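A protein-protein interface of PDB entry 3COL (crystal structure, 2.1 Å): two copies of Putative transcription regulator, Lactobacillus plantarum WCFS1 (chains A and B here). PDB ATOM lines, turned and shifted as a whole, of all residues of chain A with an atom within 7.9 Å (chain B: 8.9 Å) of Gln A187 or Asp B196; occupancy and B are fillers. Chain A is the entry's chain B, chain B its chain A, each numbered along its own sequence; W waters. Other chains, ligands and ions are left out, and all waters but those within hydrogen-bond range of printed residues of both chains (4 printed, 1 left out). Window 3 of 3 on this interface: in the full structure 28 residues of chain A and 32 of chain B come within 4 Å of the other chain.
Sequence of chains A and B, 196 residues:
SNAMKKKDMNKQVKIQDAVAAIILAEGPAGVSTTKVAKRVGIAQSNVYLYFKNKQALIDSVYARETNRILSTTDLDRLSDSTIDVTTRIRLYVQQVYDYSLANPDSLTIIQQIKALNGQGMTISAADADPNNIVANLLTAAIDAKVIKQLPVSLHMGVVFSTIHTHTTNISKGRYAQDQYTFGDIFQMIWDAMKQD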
ATOM      1  N   VAL A  93      -4.662  -6.251   9.025  1.00  0.00           N
ATOM      2  CA  VAL A  93      -3.313  -5.821   8.576  1.00  0.00           C
ATOM      3  C   VAL A  93      -3.262  -4.314   8.333  1.00  0.00           C
ATOM      4  O   VAL A  93      -2.273  -3.641   8.706  1.00  0.00           O
ATOM      5  CB  VAL A  93      -2.813  -6.607   7.325  1.00  0.00           C
ATOM      6  CG1 VAL A  93      -1.483  -6.032   6.794  1.00  0.00           C
ATOM      7  CG2 VAL A  93      -2.664  -8.109   7.628  1.00  0.00           C
ATOM      8  N   THR A 162       7.230  -7.132   8.191  1.00  0.00           N
ATOM      9  CA  THR A 162       7.167  -6.325   6.957  1.00  0.00           C
ATOM     10  C   THR A 162       6.769  -4.870   7.276  1.00  0.00           C
ATOM     11  O   THR A 162       7.419  -3.900   6.829  1.00  0.00           O
ATOM     12  CB  THR A 162       6.179  -6.932   5.950  1.00  0.00           C
ATOM     13  OG1 THR A 162       6.631  -8.241   5.619  1.00  0.00           O
ATOM     14  CG2 THR A 162       6.126  -6.146   4.655  1.00  0.00           C
ATOM     15  N   THR A 181       2.179   2.742  -1.126  1.00  0.00           N
ATOM     16  CA  THR A 181       0.817   2.686  -0.599  1.00  0.00           C
ATOM     17  C   THR A 181       0.652   1.423   0.264  1.00  0.00           C
ATOM     18  O   THR A 181       1.492   0.500   0.198  1.00  0.00           O
ATOM     19  CB  THR A 181      -0.234   2.552  -1.722  1.00  0.00           C
ATOM     20  OG1 THR A 181       0.076   1.392  -2.485  1.00  0.00           O
ATOM     21  CG2 THR A 181      -0.293   3.783  -2.662  1.00  0.00           C
ATOM     22  N   PHE A 182      -0.427   1.377   1.057  1.00  0.00           N
ATOM     23  CA  PHE A 182      -0.794   0.146   1.769  1.00  0.00           C
ATOM     24  C   PHE A 182      -0.946  -1.017   0.764  1.00  0.00           C
ATOM     25  O   PHE A 182      -0.424  -2.124   0.986  1.00  0.00           O
ATOM     26  CB  PHE A 182      -2.095   0.331   2.576  1.00  0.00           C
ATOM     27  CG  PHE A 182      -2.587  -0.944   3.160  1.00  0.00           C
ATOM     28  CD1 PHE A 182      -1.871  -1.585   4.161  1.00  0.00           C
ATOM     29  CD2 PHE A 182      -3.711  -1.557   2.656  1.00  0.00           C
ATOM     30  CE1 PHE A 182      -2.304  -2.800   4.672  1.00  0.00           C
ATOM     31  CE2 PHE A 182      -4.146  -2.764   3.169  1.00  0.00           C
ATOM     32  CZ  PHE A 182      -3.453  -3.372   4.174  1.00  0.00           C
ATOM     33  N   GLY A 183      -1.638  -0.747  -0.350  1.00  0.00           N
ATOM     34  CA  GLY A 183      -1.707  -1.691  -1.495  1.00  0.00           C
ATOM     35  C   GLY A 183      -0.348  -2.315  -1.840  1.00  0.00           C
ATOM     36  O   GLY A 183      -0.241  -3.526  -2.029  1.00  0.00           O
ATOM     37  N   ASP A 184       0.702  -1.500  -1.938  1.00  0.00           N
ATOM     38  CA  ASP A 184       2.021  -2.028  -2.359  1.00  0.00           C
ATOM     39  C   ASP A 184       2.607  -3.004  -1.318  1.00  0.00           C
ATOM     40  O   ASP A 184       3.166  -4.070  -1.656  1.00  0.00           O
ATOM     41  CB  ASP A 184       3.016  -0.889  -2.588  1.00  0.00           C
ATOM     42  CG  ASP A 184       2.636   0.009  -3.755  1.00  0.00           C
ATOM     43  OD1 ASP A 184       2.126  -0.500  -4.769  1.00  0.00           O
ATOM     44  OD2 ASP A 184       2.888   1.234  -3.674  1.00  0.00           O
ATOM     45  N   ILE A 185       2.525  -2.605  -0.060  1.00  0.00           N
ATOM     46  CA  ILE A 185       3.106  -3.387   1.025  1.00  0.00           C
ATOM     47  C   ILE A 185       2.219  -4.624   1.296  1.00  0.00           C
ATOM     48  O   ILE A 185       2.726  -5.726   1.489  1.00  0.00           O
ATOM     49  CB  ILE A 185       3.238  -2.531   2.315  1.00  0.00           C
ATOM     50  CG1 ILE A 185       4.007  -1.232   2.034  1.00  0.00           C
ATOM     51  CG2 ILE A 185       3.868  -3.357   3.515  1.00  0.00           C
ATOM     52  CD1 ILE A 185       5.411  -1.420   1.480  1.00  0.00           C
ATOM     53  N   PHE A 186       0.899  -4.415   1.322  1.00  0.00           N
ATOM     54  CA  PHE A 186      -0.048  -5.522   1.492  1.00  0.00           C
ATOM     55  C   PHE A 186       0.116  -6.618   0.445  1.00  0.00           C
ATOM     56  O   PHE A 186      -0.100  -7.814   0.727  1.00  0.00           O
ATOM     57  CB  PHE A 186      -1.507  -5.031   1.526  1.00  0.00           C
ATOM     58  CG  PHE A 186      -2.491  -6.110   1.972  1.00  0.00           C
ATOM     59  CD1 PHE A 186      -2.358  -6.715   3.227  1.00  0.00           C
ATOM     60  CD2 PHE A 186      -3.492  -6.561   1.113  1.00  0.00           C
ATOM     61  CE1 PHE A 186      -3.265  -7.742   3.643  1.00  0.00           C
ATOM     62  CE2 PHE A 186      -4.385  -7.577   1.512  1.00  0.00           C
ATOM     63  CZ  PHE A 186      -4.270  -8.155   2.781  1.00  0.00           C
ATOM     64  N   GLN A 187       0.473  -6.252  -0.779  1.00  0.00           N
ATOM     65  CA  GLN A 187       0.677  -7.294  -1.778  1.00  0.00           C
ATOM     66  C   GLN A 187       1.752  -8.319  -1.374  1.00  0.00           C
ATOM     67  O   GLN A 187       1.583  -9.511  -1.552  1.00  0.00           O
ATOM     68  CB  GLN A 187       0.966  -6.683  -3.132  1.00  0.00           C
ATOM     69  CG  GLN A 187       0.766  -7.680  -4.306  1.00  0.00           C
ATOM     70  CD  GLN A 187       1.179  -7.078  -5.627  1.00  0.00           C
ATOM     71  OE1 GLN A 187       2.282  -6.528  -5.771  1.00  0.00           O
ATOM     72  NE2 GLN A 187       0.292  -7.171  -6.612  1.00  0.00           N
ATOM     73  N   MET A 188       2.846  -7.857  -0.797  1.00  0.00           N
ATOM     74  CA  MET A 188       3.872  -8.762  -0.304  1.00  0.00           C
ATOM     75  C   MET A 188       3.303  -9.604   0.836  1.00  0.00           C
ATOM     76  O   MET A 188       3.517 -10.808   0.894  1.00  0.00           O
ATOM     77  CB  MET A 188       5.088  -7.966   0.186  1.00  0.00           C
ATOM     78  CG  MET A 188       6.104  -8.821   0.997  1.00  0.00           C
ATOM     79  SD  MET A 188       7.757  -7.900   1.393  1.00  0.00           S
ATOM     80  CE  MET A 188       8.757  -8.265  -0.226  1.00  0.00           C
ATOM     81  N   ILE A 189       2.599  -8.950   1.752  1.00  0.00           N
ATOM     82  CA  ILE A 189       2.131  -9.601   2.960  1.00  0.00           C
ATOM     83  C   ILE A 189       1.069 -10.638   2.637  1.00  0.00           C
ATOM     84  O   ILE A 189       1.162 -11.778   3.092  1.00  0.00           O
ATOM     85  CB  ILE A 189       1.611  -8.574   4.016  1.00  0.00           C
ATOM     86  CG1 ILE A 189       2.818  -7.752   4.554  1.00  0.00           C
ATOM     87  CG2 ILE A 189       0.861  -9.327   5.162  1.00  0.00           C
ATOM     88  CD1 ILE A 189       2.435  -6.497   5.408  1.00  0.00           C
ATOM     89  N   TRP A 190       0.072 -10.253   1.838  1.00  0.00           N
ATOM     90  CA  TRP A 190      -0.977 -11.195   1.451  1.00  0.00           C
ATOM     91  C   TRP A 190      -0.466 -12.335   0.540  1.00  0.00           C
ATOM     92  O   TRP A 190      -0.932 -13.473   0.652  1.00  0.00           O
ATOM     93  CB  TRP A 190      -2.147 -10.447   0.784  1.00  0.00           C
ATOM     94  CG  TRP A 190      -3.303 -11.301   0.423  1.00  0.00           C
ATOM     95  CD1 TRP A 190      -3.872 -11.459  -0.847  1.00  0.00           C
ATOM     96  CD2 TRP A 190      -4.086 -12.107   1.315  1.00  0.00           C
ATOM     97  NE1 TRP A 190      -4.945 -12.326  -0.764  1.00  0.00           N
ATOM     98  CE2 TRP A 190      -5.105 -12.724   0.542  1.00  0.00           C
ATOM     99  CE3 TRP A 190      -4.044 -12.352   2.696  1.00  0.00           C
ATOM    100  CZ2 TRP A 190      -6.042 -13.585   1.104  1.00  0.00           C
ATOM    101  CZ3 TRP A 190      -4.991 -13.211   3.242  1.00  0.00           C
ATOM    102  CH2 TRP A 190      -5.958 -13.813   2.449  1.00  0.00           C
ATOM    103  N   ASP A 191       0.458 -12.022  -0.367  1.00  0.00           N
ATOM    104  CA  ASP A 191       1.041 -13.072  -1.217  1.00  0.00           C
ATOM    105  C   ASP A 191       1.735 -14.092  -0.304  1.00  0.00           C
ATOM    106  O   ASP A 191       1.600 -15.301  -0.497  1.00  0.00           O
ATOM    107  CB  ASP A 191       2.065 -12.492  -2.193  1.00  0.00           C
ATOM    108  CG  ASP A 191       1.422 -11.853  -3.430  1.00  0.00           C
ATOM    109  OD1 ASP A 191       0.188 -11.938  -3.613  1.00  0.00           O
ATOM    110  OD2 ASP A 191       2.177 -11.289  -4.242  1.00  0.00           O
ATOM    111  N   ALA A 192       2.450 -13.583   0.707  1.00  0.00           N
ATOM    112  CA  ALA A 192       3.110 -14.444   1.697  1.00  0.00           C
ATOM    113  C   ALA A 192       2.137 -15.389   2.396  1.00  0.00           C
ATOM    114  O   ALA A 192       2.357 -16.604   2.438  1.00  0.00           O
ATOM    115  CB  ALA A 192       3.897 -13.600   2.705  1.00  0.00           C
ATOM    116  N   MET A 193       1.019 -14.852   2.863  1.00  0.00           N
ATOM    117  CA  MET A 193       0.034 -15.590   3.627  1.00  0.00           C
ATOM    118  C   MET A 193      -0.853 -16.575   2.820  1.00  0.00           C
ATOM    119  O   MET A 193      -1.088 -17.696   3.261  1.00  0.00           O
ATOM    120  CB  MET A 193      -0.866 -14.604   4.393  1.00  0.00           C
ATOM    121  CG  MET A 193      -0.121 -13.684   5.405  1.00  0.00           C
ATOM    122  SD  MET A 193      -1.383 -12.482   6.180  1.00  0.00           S
ATOM    123  CE  MET A 193      -2.353 -13.782   7.332  1.00  0.00           C
ATOM    124  N   LYS A 194      -1.330 -16.159   1.645  1.00  0.00           N
ATOM    125  CA  LYS A 194      -2.432 -16.855   0.982  1.00  0.00           C
ATOM    126  C   LYS A 194      -2.059 -18.191   0.378  1.00  0.00           C
ATOM    127  O   LYS A 194      -0.916 -18.443   0.027  1.00  0.00           O
ATOM    128  CB  LYS A 194      -3.158 -15.971  -0.051  1.00  0.00           C
ATOM    129  CG  LYS A 194      -2.399 -15.733  -1.365  1.00  0.00           C
ATOM    130  CD  LYS A 194      -3.188 -14.761  -2.301  1.00  0.00           C
ATOM    131  CE  LYS A 194      -2.374 -14.392  -3.536  1.00  0.00           C
ATOM    132  NZ  LYS A 194      -2.289 -15.611  -4.384  1.00  0.00           N
ATOM    133  N   LYS B 145      11.956  -7.465 -13.302  1.00  0.00           N
ATOM    134  CA  LYS B 145      10.588  -7.691 -12.879  1.00  0.00           C
ATOM    135  C   LYS B 145      10.312  -9.142 -12.437  1.00  0.00           C
ATOM    136  O   LYS B 145       9.199  -9.646 -12.574  1.00  0.00           O
ATOM    137  CB  LYS B 145       9.585  -7.162 -13.919  1.00  0.00           C
ATOM    138  CG  LYS B 145       9.644  -5.621 -14.074  1.00  0.00           C
ATOM    139  CD  LYS B 145       8.284  -5.022 -14.504  1.00  0.00           C
ATOM    140  CE  LYS B 145       8.309  -3.484 -14.599  1.00  0.00           C
ATOM    141  NZ  LYS B 145       7.377  -2.971 -15.702  1.00  0.00           N
ATOM    142  N   VAL B 146      11.343  -9.773 -11.884  1.00  0.00           N
ATOM    143  CA  VAL B 146      11.240 -11.111 -11.320  1.00  0.00           C
ATOM    144  C   VAL B 146      10.697 -11.052  -9.893  1.00  0.00           C
ATOM    145  O   VAL B 146       9.865 -11.882  -9.495  1.00  0.00           O
ATOM    146  CB  VAL B 146      12.603 -11.806 -11.381  1.00  0.00           C
ATOM    147  CG1 VAL B 146      12.634 -13.044 -10.535  1.00  0.00           C
ATOM    148  CG2 VAL B 146      12.926 -12.167 -12.868  1.00  0.00           C
ATOM    149  N   ILE B 147      11.171 -10.096  -9.102  1.00  0.00           N
ATOM    150  CA  ILE B 147      10.591  -9.895  -7.769  1.00  0.00           C
ATOM    151  C   ILE B 147       9.977  -8.487  -7.696  1.00  0.00           C
ATOM    152  O   ILE B 147      10.239  -7.638  -8.580  1.00  0.00           O
ATOM    153  CB  ILE B 147      11.624 -10.158  -6.643  1.00  0.00           C
ATOM    154  CG1 ILE B 147      12.706  -9.064  -6.658  1.00  0.00           C
ATOM    155  CG2 ILE B 147      12.147 -11.613  -6.732  1.00  0.00           C
ATOM    156  CD1 ILE B 147      13.857  -9.226  -5.618  1.00  0.00           C
ATOM    157  N   LYS B 148       9.141  -8.261  -6.689  1.00  0.00           N
ATOM    158  CA  LYS B 148       8.374  -7.026  -6.538  1.00  0.00           C
ATOM    159  C   LYS B 148       9.194  -5.731  -6.526  1.00  0.00           C
ATOM    160  O   LYS B 148      10.312  -5.691  -5.999  1.00  0.00           O
ATOM    161  CB  LYS B 148       7.535  -7.099  -5.259  1.00  0.00           C
ATOM    162  CG  LYS B 148       6.428  -8.186  -5.319  1.00  0.00           C
ATOM    163  CD  LYS B 148       5.520  -8.138  -4.078  1.00  0.00           C
ATOM    164  CE  LYS B 148       4.292  -9.037  -4.206  1.00  0.00           C
ATOM    165  NZ  LYS B 148       4.742 -10.489  -4.120  1.00  0.00           N
ATOM    166  N   GLN B 149       8.633  -4.663  -7.096  1.00  0.00           N
ATOM    167  CA  GLN B 149       9.295  -3.345  -7.052  1.00  0.00           C
ATOM    168  C   GLN B 149       9.173  -2.778  -5.651  1.00  0.00           C
ATOM    169  O   GLN B 149       8.430  -1.831  -5.418  1.00  0.00           O
ATOM    170  CB  GLN B 149       8.667  -2.351  -8.068  1.00  0.00           C
ATOM    171  CG  GLN B 149       8.652  -2.856  -9.492  1.00  0.00           C
ATOM    172  CD  GLN B 149      10.048  -3.091 -10.031  1.00  0.00           C
ATOM    173  OE1 GLN B 149      10.339  -4.168 -10.561  1.00  0.00           O
ATOM    174  NE2 GLN B 149      10.937  -2.093  -9.861  1.00  0.00           N
ATOM    175  N   LEU B 150       9.849  -3.403  -4.690  1.00  0.00           N
ATOM    176  CA  LEU B 150       9.830  -2.955  -3.328  1.00  0.00           C
ATOM    177  C   LEU B 150      11.274  -2.869  -2.871  1.00  0.00           C
ATOM    178  O   LEU B 150      12.161  -3.469  -3.492  1.00  0.00           O
ATOM    179  CB  LEU B 150       9.069  -3.964  -2.441  1.00  0.00           C
ATOM    180  CG  LEU B 150       7.531  -4.011  -2.593  1.00  0.00           C
ATOM    181  CD1 LEU B 150       6.954  -5.184  -1.823  1.00  0.00           C
ATOM    182  CD2 LEU B 150       6.893  -2.684  -2.144  1.00  0.00           C
ATOM    183  N   LEU B 154      12.944  -4.788   2.331  1.00  0.00           N
ATOM    184  CA  LEU B 154      11.702  -5.547   2.529  1.00  0.00           C
ATOM    185  C   LEU B 154      11.806  -7.012   2.095  1.00  0.00           C
ATOM    186  O   LEU B 154      11.290  -7.907   2.766  1.00  0.00           O
ATOM    187  CB  LEU B 154      10.500  -4.903   1.829  1.00  0.00           C
ATOM    188  CG  LEU B 154       9.882  -3.583   2.308  1.00  0.00           C
ATOM    189  CD1 LEU B 154       8.337  -3.551   2.132  1.00  0.00           C
ATOM    190  CD2 LEU B 154      10.212  -3.289   3.667  1.00  0.00           C
ATOM    191  N   MET B 188       6.120 -19.532   1.324  1.00  0.00           N
ATOM    192  CA  MET B 188       5.720 -18.223   1.888  1.00  0.00           C
ATOM    193  C   MET B 188       6.703 -17.085   1.477  1.00  0.00           C
ATOM    194  O   MET B 188       6.287 -16.027   1.010  1.00  0.00           O
ATOM    195  CB  MET B 188       5.581 -18.293   3.407  1.00  0.00           C
ATOM    196  CG  MET B 188       5.676 -16.877   4.048  1.00  0.00           C
ATOM    197  SD  MET B 188       5.301 -16.936   5.954  1.00  0.00           S
ATOM    198  CE  MET B 188       3.361 -16.959   5.979  1.00  0.00           C
ATOM    199  N   TRP B 190       9.027 -16.937  -1.008  1.00  0.00           N
ATOM    200  CA  TRP B 190       9.068 -16.704  -2.457  1.00  0.00           C
ATOM    201  C   TRP B 190       7.803 -16.025  -2.977  1.00  0.00           C
ATOM    202  O   TRP B 190       7.889 -15.119  -3.804  1.00  0.00           O
ATOM    203  CB  TRP B 190       9.364 -18.022  -3.253  1.00  0.00           C
ATOM    204  CG  TRP B 190       9.477 -17.825  -4.785  1.00  0.00           C
ATOM    205  CD1 TRP B 190       8.726 -18.451  -5.755  1.00  0.00           C
ATOM    206  CD2 TRP B 190      10.375 -16.936  -5.498  1.00  0.00           C
ATOM    207  NE1 TRP B 190       9.105 -18.018  -6.997  1.00  0.00           N
ATOM    208  CE2 TRP B 190      10.096 -17.080  -6.876  1.00  0.00           C
ATOM    209  CE3 TRP B 190      11.365 -16.007  -5.096  1.00  0.00           C
ATOM    210  CZ2 TRP B 190      10.793 -16.360  -7.864  1.00  0.00           C
ATOM    211  CZ3 TRP B 190      12.044 -15.287  -6.065  1.00  0.00           C
ATOM    212  CH2 TRP B 190      11.759 -15.458  -7.439  1.00  0.00           C
ATOM    213  N   ASP B 191       6.628 -16.482  -2.540  1.00  0.00           N
ATOM    214  CA  ASP B 191       5.366 -15.735  -2.821  1.00  0.00           C
ATOM    215  C   ASP B 191       5.446 -14.251  -2.397  1.00  0.00           C
ATOM    216  O   ASP B 191       5.009 -13.348  -3.142  1.00  0.00           O
ATOM    217  CB  ASP B 191       4.147 -16.385  -2.139  1.00  0.00           C
ATOM    218  CG  ASP B 191       3.764 -17.712  -2.774  1.00  0.00           C
ATOM    219  OD1 ASP B 191       4.359 -18.043  -3.812  1.00  0.00           O
ATOM    220  OD2 ASP B 191       2.880 -18.424  -2.239  1.00  0.00           O
ATOM    221  N   ALA B 192       5.955 -14.019  -1.185  1.00  0.00           N
ATOM    222  CA  ALA B 192       6.119 -12.634  -0.648  1.00  0.00           C
ATOM    223  C   ALA B 192       6.956 -11.812  -1.622  1.00  0.00           C
ATOM    224  O   ALA B 192       6.564 -10.735  -1.992  1.00  0.00           O
ATOM    225  CB  ALA B 192       6.806 -12.664   0.671  1.00  0.00           C
ATOM    226  N   MET B 193       8.092 -12.356  -2.054  1.00  0.00           N
ATOM    227  CA  MET B 193       9.035 -11.643  -2.935  1.00  0.00           C
ATOM    228  C   MET B 193       8.619 -11.505  -4.413  1.00  0.00           C
ATOM    229  O   MET B 193       8.882 -10.487  -5.036  1.00  0.00           O
ATOM    230  CB  MET B 193      10.413 -12.346  -2.922  1.00  0.00           C
ATOM    231  CG  MET B 193      11.095 -12.454  -1.535  1.00  0.00           C
ATOM    232  SD  MET B 193      12.711 -13.498  -1.637  1.00  0.00           S
ATOM    233  CE  MET B 193      13.946 -12.206  -2.438  1.00  0.00           C
ATOM    234  N   LYS B 194       8.057 -12.552  -4.993  1.00  0.00           N
ATOM    235  CA  LYS B 194       7.975 -12.638  -6.448  1.00  0.00           C
ATOM    236  C   LYS B 194       6.975 -11.677  -7.061  1.00  0.00           C
ATOM    237  O   LYS B 194       5.983 -11.314  -6.441  1.00  0.00           O
ATOM    238  CB  LYS B 194       7.764 -14.078  -6.937  1.00  0.00           C
ATOM    239  CG  LYS B 194       6.346 -14.589  -6.852  1.00  0.00           C
ATOM    240  CD  LYS B 194       6.236 -15.958  -7.524  1.00  0.00           C
ATOM    241  CE  LYS B 194       5.106 -16.770  -6.916  1.00  0.00           C
ATOM    242  NZ  LYS B 194       3.842 -16.132  -7.330  1.00  0.00           N
ATOM    243  N   GLN B 195       7.272 -11.251  -8.287  1.00  0.00           N
ATOM    244  CA  GLN B 195       6.500 -10.221  -8.956  1.00  0.00           C
ATOM    245  C   GLN B 195       5.109 -10.770  -9.358  1.00  0.00           C
ATOM    246  O   GLN B 195       5.015 -11.812  -9.989  1.00  0.00           O
ATOM    247  CB  GLN B 195       7.302  -9.697 -10.135  1.00  0.00           C
ATOM    248  CG  GLN B 195       6.501  -8.940 -11.195  1.00  0.00           C
ATOM    249  CD  GLN B 195       6.026  -7.586 -10.694  1.00  0.00           C
ATOM    250  OE1 GLN B 195       6.820  -6.768 -10.209  1.00  0.00           O
ATOM    251  NE2 GLN B 195       4.724  -7.336 -10.831  1.00  0.00           N
ATOM    252  N   ASP B 196       4.062 -10.028  -8.969  1.00  0.00           N
ATOM    253  CA  ASP B 196       2.633 -10.445  -8.863  1.00  0.00           C
ATOM    254  C   ASP B 196       2.243 -11.030  -7.476  1.00  0.00           C
ATOM    255  O   ASP B 196       2.560 -12.193  -7.203  1.00  0.00           O
ATOM    256  CB  ASP B 196       2.259 -11.407  -9.955  1.00  0.00           C
ATOM    257  CG  ASP B 196       2.173 -10.742 -11.316  1.00  0.00           C
ATOM    258  OD1 ASP B 196       1.462 -11.303 -12.168  1.00  0.00           O
ATOM    259  OD2 ASP B 196       2.807  -9.682 -11.527  1.00  0.00           O
ATOM    260  OXT ASP B 196       1.598 -10.392  -6.611  1.00  0.00           O
HETATM  261  O   HOH W   1       3.762  -7.650  -8.060  1.00  0.00           O
HETATM  262  O   HOH W   2       9.674  -7.479   4.845  1.00  0.00           O
HETATM  263  O   HOH W   3       5.067  -2.185  -5.442  1.00  0.00           O
HETATM  264  O   HOH W   4       0.493 -16.228  -2.803  1.00  0.00           O
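The side-chain amino group (NZ) of Lys B148 is in salt-bridge range of the side-chain carboxylate (OD2) of Asp A191 (2.7 Å). NE2 of Gln A187 sits at hydrogen-bond distance from OXT of Asp B196. The chain-end carboxylate of Asp B196 sits close to the side-chain carboxylate of Asp A191 (2.6 Å). The side-chain sulfur of Met A188 sits close to the backbone carbonyl oxygen of Leu B154.
The side-chain amino group (NZ) of Lys B148 sits at hydrogen-bond distance from the backbone carbonyl oxygen (O) of Asp B191, 3.0 Å away. The backbone carbonyl oxygen of Ala B192 lies within hydrogen-bond range of the side-chain amino group of Lys B148, at 2.8 Å. N of Lys B148 lies within hydrogen-bond range of O of Met B193 (2.8 Å). The side-chain amino group (NZ) of Lys B148 sits at hydrogen-bond distance from the backbone carbonyl oxygen (O) of Lys B194 (2.8 Å). The side-chain amide nitrogen (NE2) of Gln B195 sits at hydrogen-bond distance from the side-chain carboxylate (OD2) of Asp B196 (3.1 Å). OG1 of Thr A181 is in hydrogen-bond range of N of Asp A184 (3.0 Å).
Among the printed residues, merely in contact across the chains: Asp A191 with Asp B191, Met A188 with Ala B192, Gln A187 with Lys B148, Ala A192 with Met B188, Ala A192 with Ala B192, Ile A185 with Leu B154, Met A188 with Lys B148, Met A188 with Leu B150 and Asp A184 with Leu B150.
Of chain B, only Lys B148 and Asp B196 come within 4 Å of Gln A187. Of chain A, only Gln A187 (3.5 Å) and Asp A191 (2.6 Å) come within 4 Å of Asp B196. Of the printed residues of chain A, Asp B191 touches Asp A191. Printed residues of chain B within 4 Å of Asp A184: Leu B150. Of the printed residues of chain B, Ala A192 touches Met B188 (3.6 Å) and Ala B192 (3.7 Å). The nearest residue of chain A that does not touch Asp B196 is Lys A194 (6.4 Å).
Of the 16 printed residues of chain A, 6 touch a printed residue of chain B. Hydrophobic or aromatic side chains of chain A within 4 Å of the printed part of chain B: Ile A185, Met A188 and Ala A192. Among the printed residues, Asp or Glu carboxylates within 4 Å of a Lys or Arg side-chain nitrogen of the other chain: Asp A191 with Lys B148 (2.7 Å).
Met A188 touches Ala B192, and with the chains exchanged Ala A192 touches Met B188. Asp A191 touches its own counterpart, Asp B191. Ala B192 touches its own counterpart, Ala A192. 6 positions are printed for both chains.
Water W1 lies within hydrogen-bond range of N of Asp B196 (2.6 Å), OE1 of Gln A187 (2.9 Å) and NE2 of Gln B195 (2.9 Å). Water W2 lies within hydrogen-bond range of the backbone carbonyl oxygen (O) of Leu B154 (2.7 Å) and the side-chain hydroxyl (OG1) of Thr A162 (3.2 Å). Water W4 lies within hydrogen-bond range of O of Asp A191 (2.7 Å), NZ of Lys A194 (3.3 Å) and OD2 of Asp B191 (3.3 Å). Water W3 lies within hydrogen-bond range of the backbone carbonyl oxygen (O) of Gln B149 (3.4 Å) and the side-chain carboxylate (OD1) of Asp A184 (3.5 Å).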
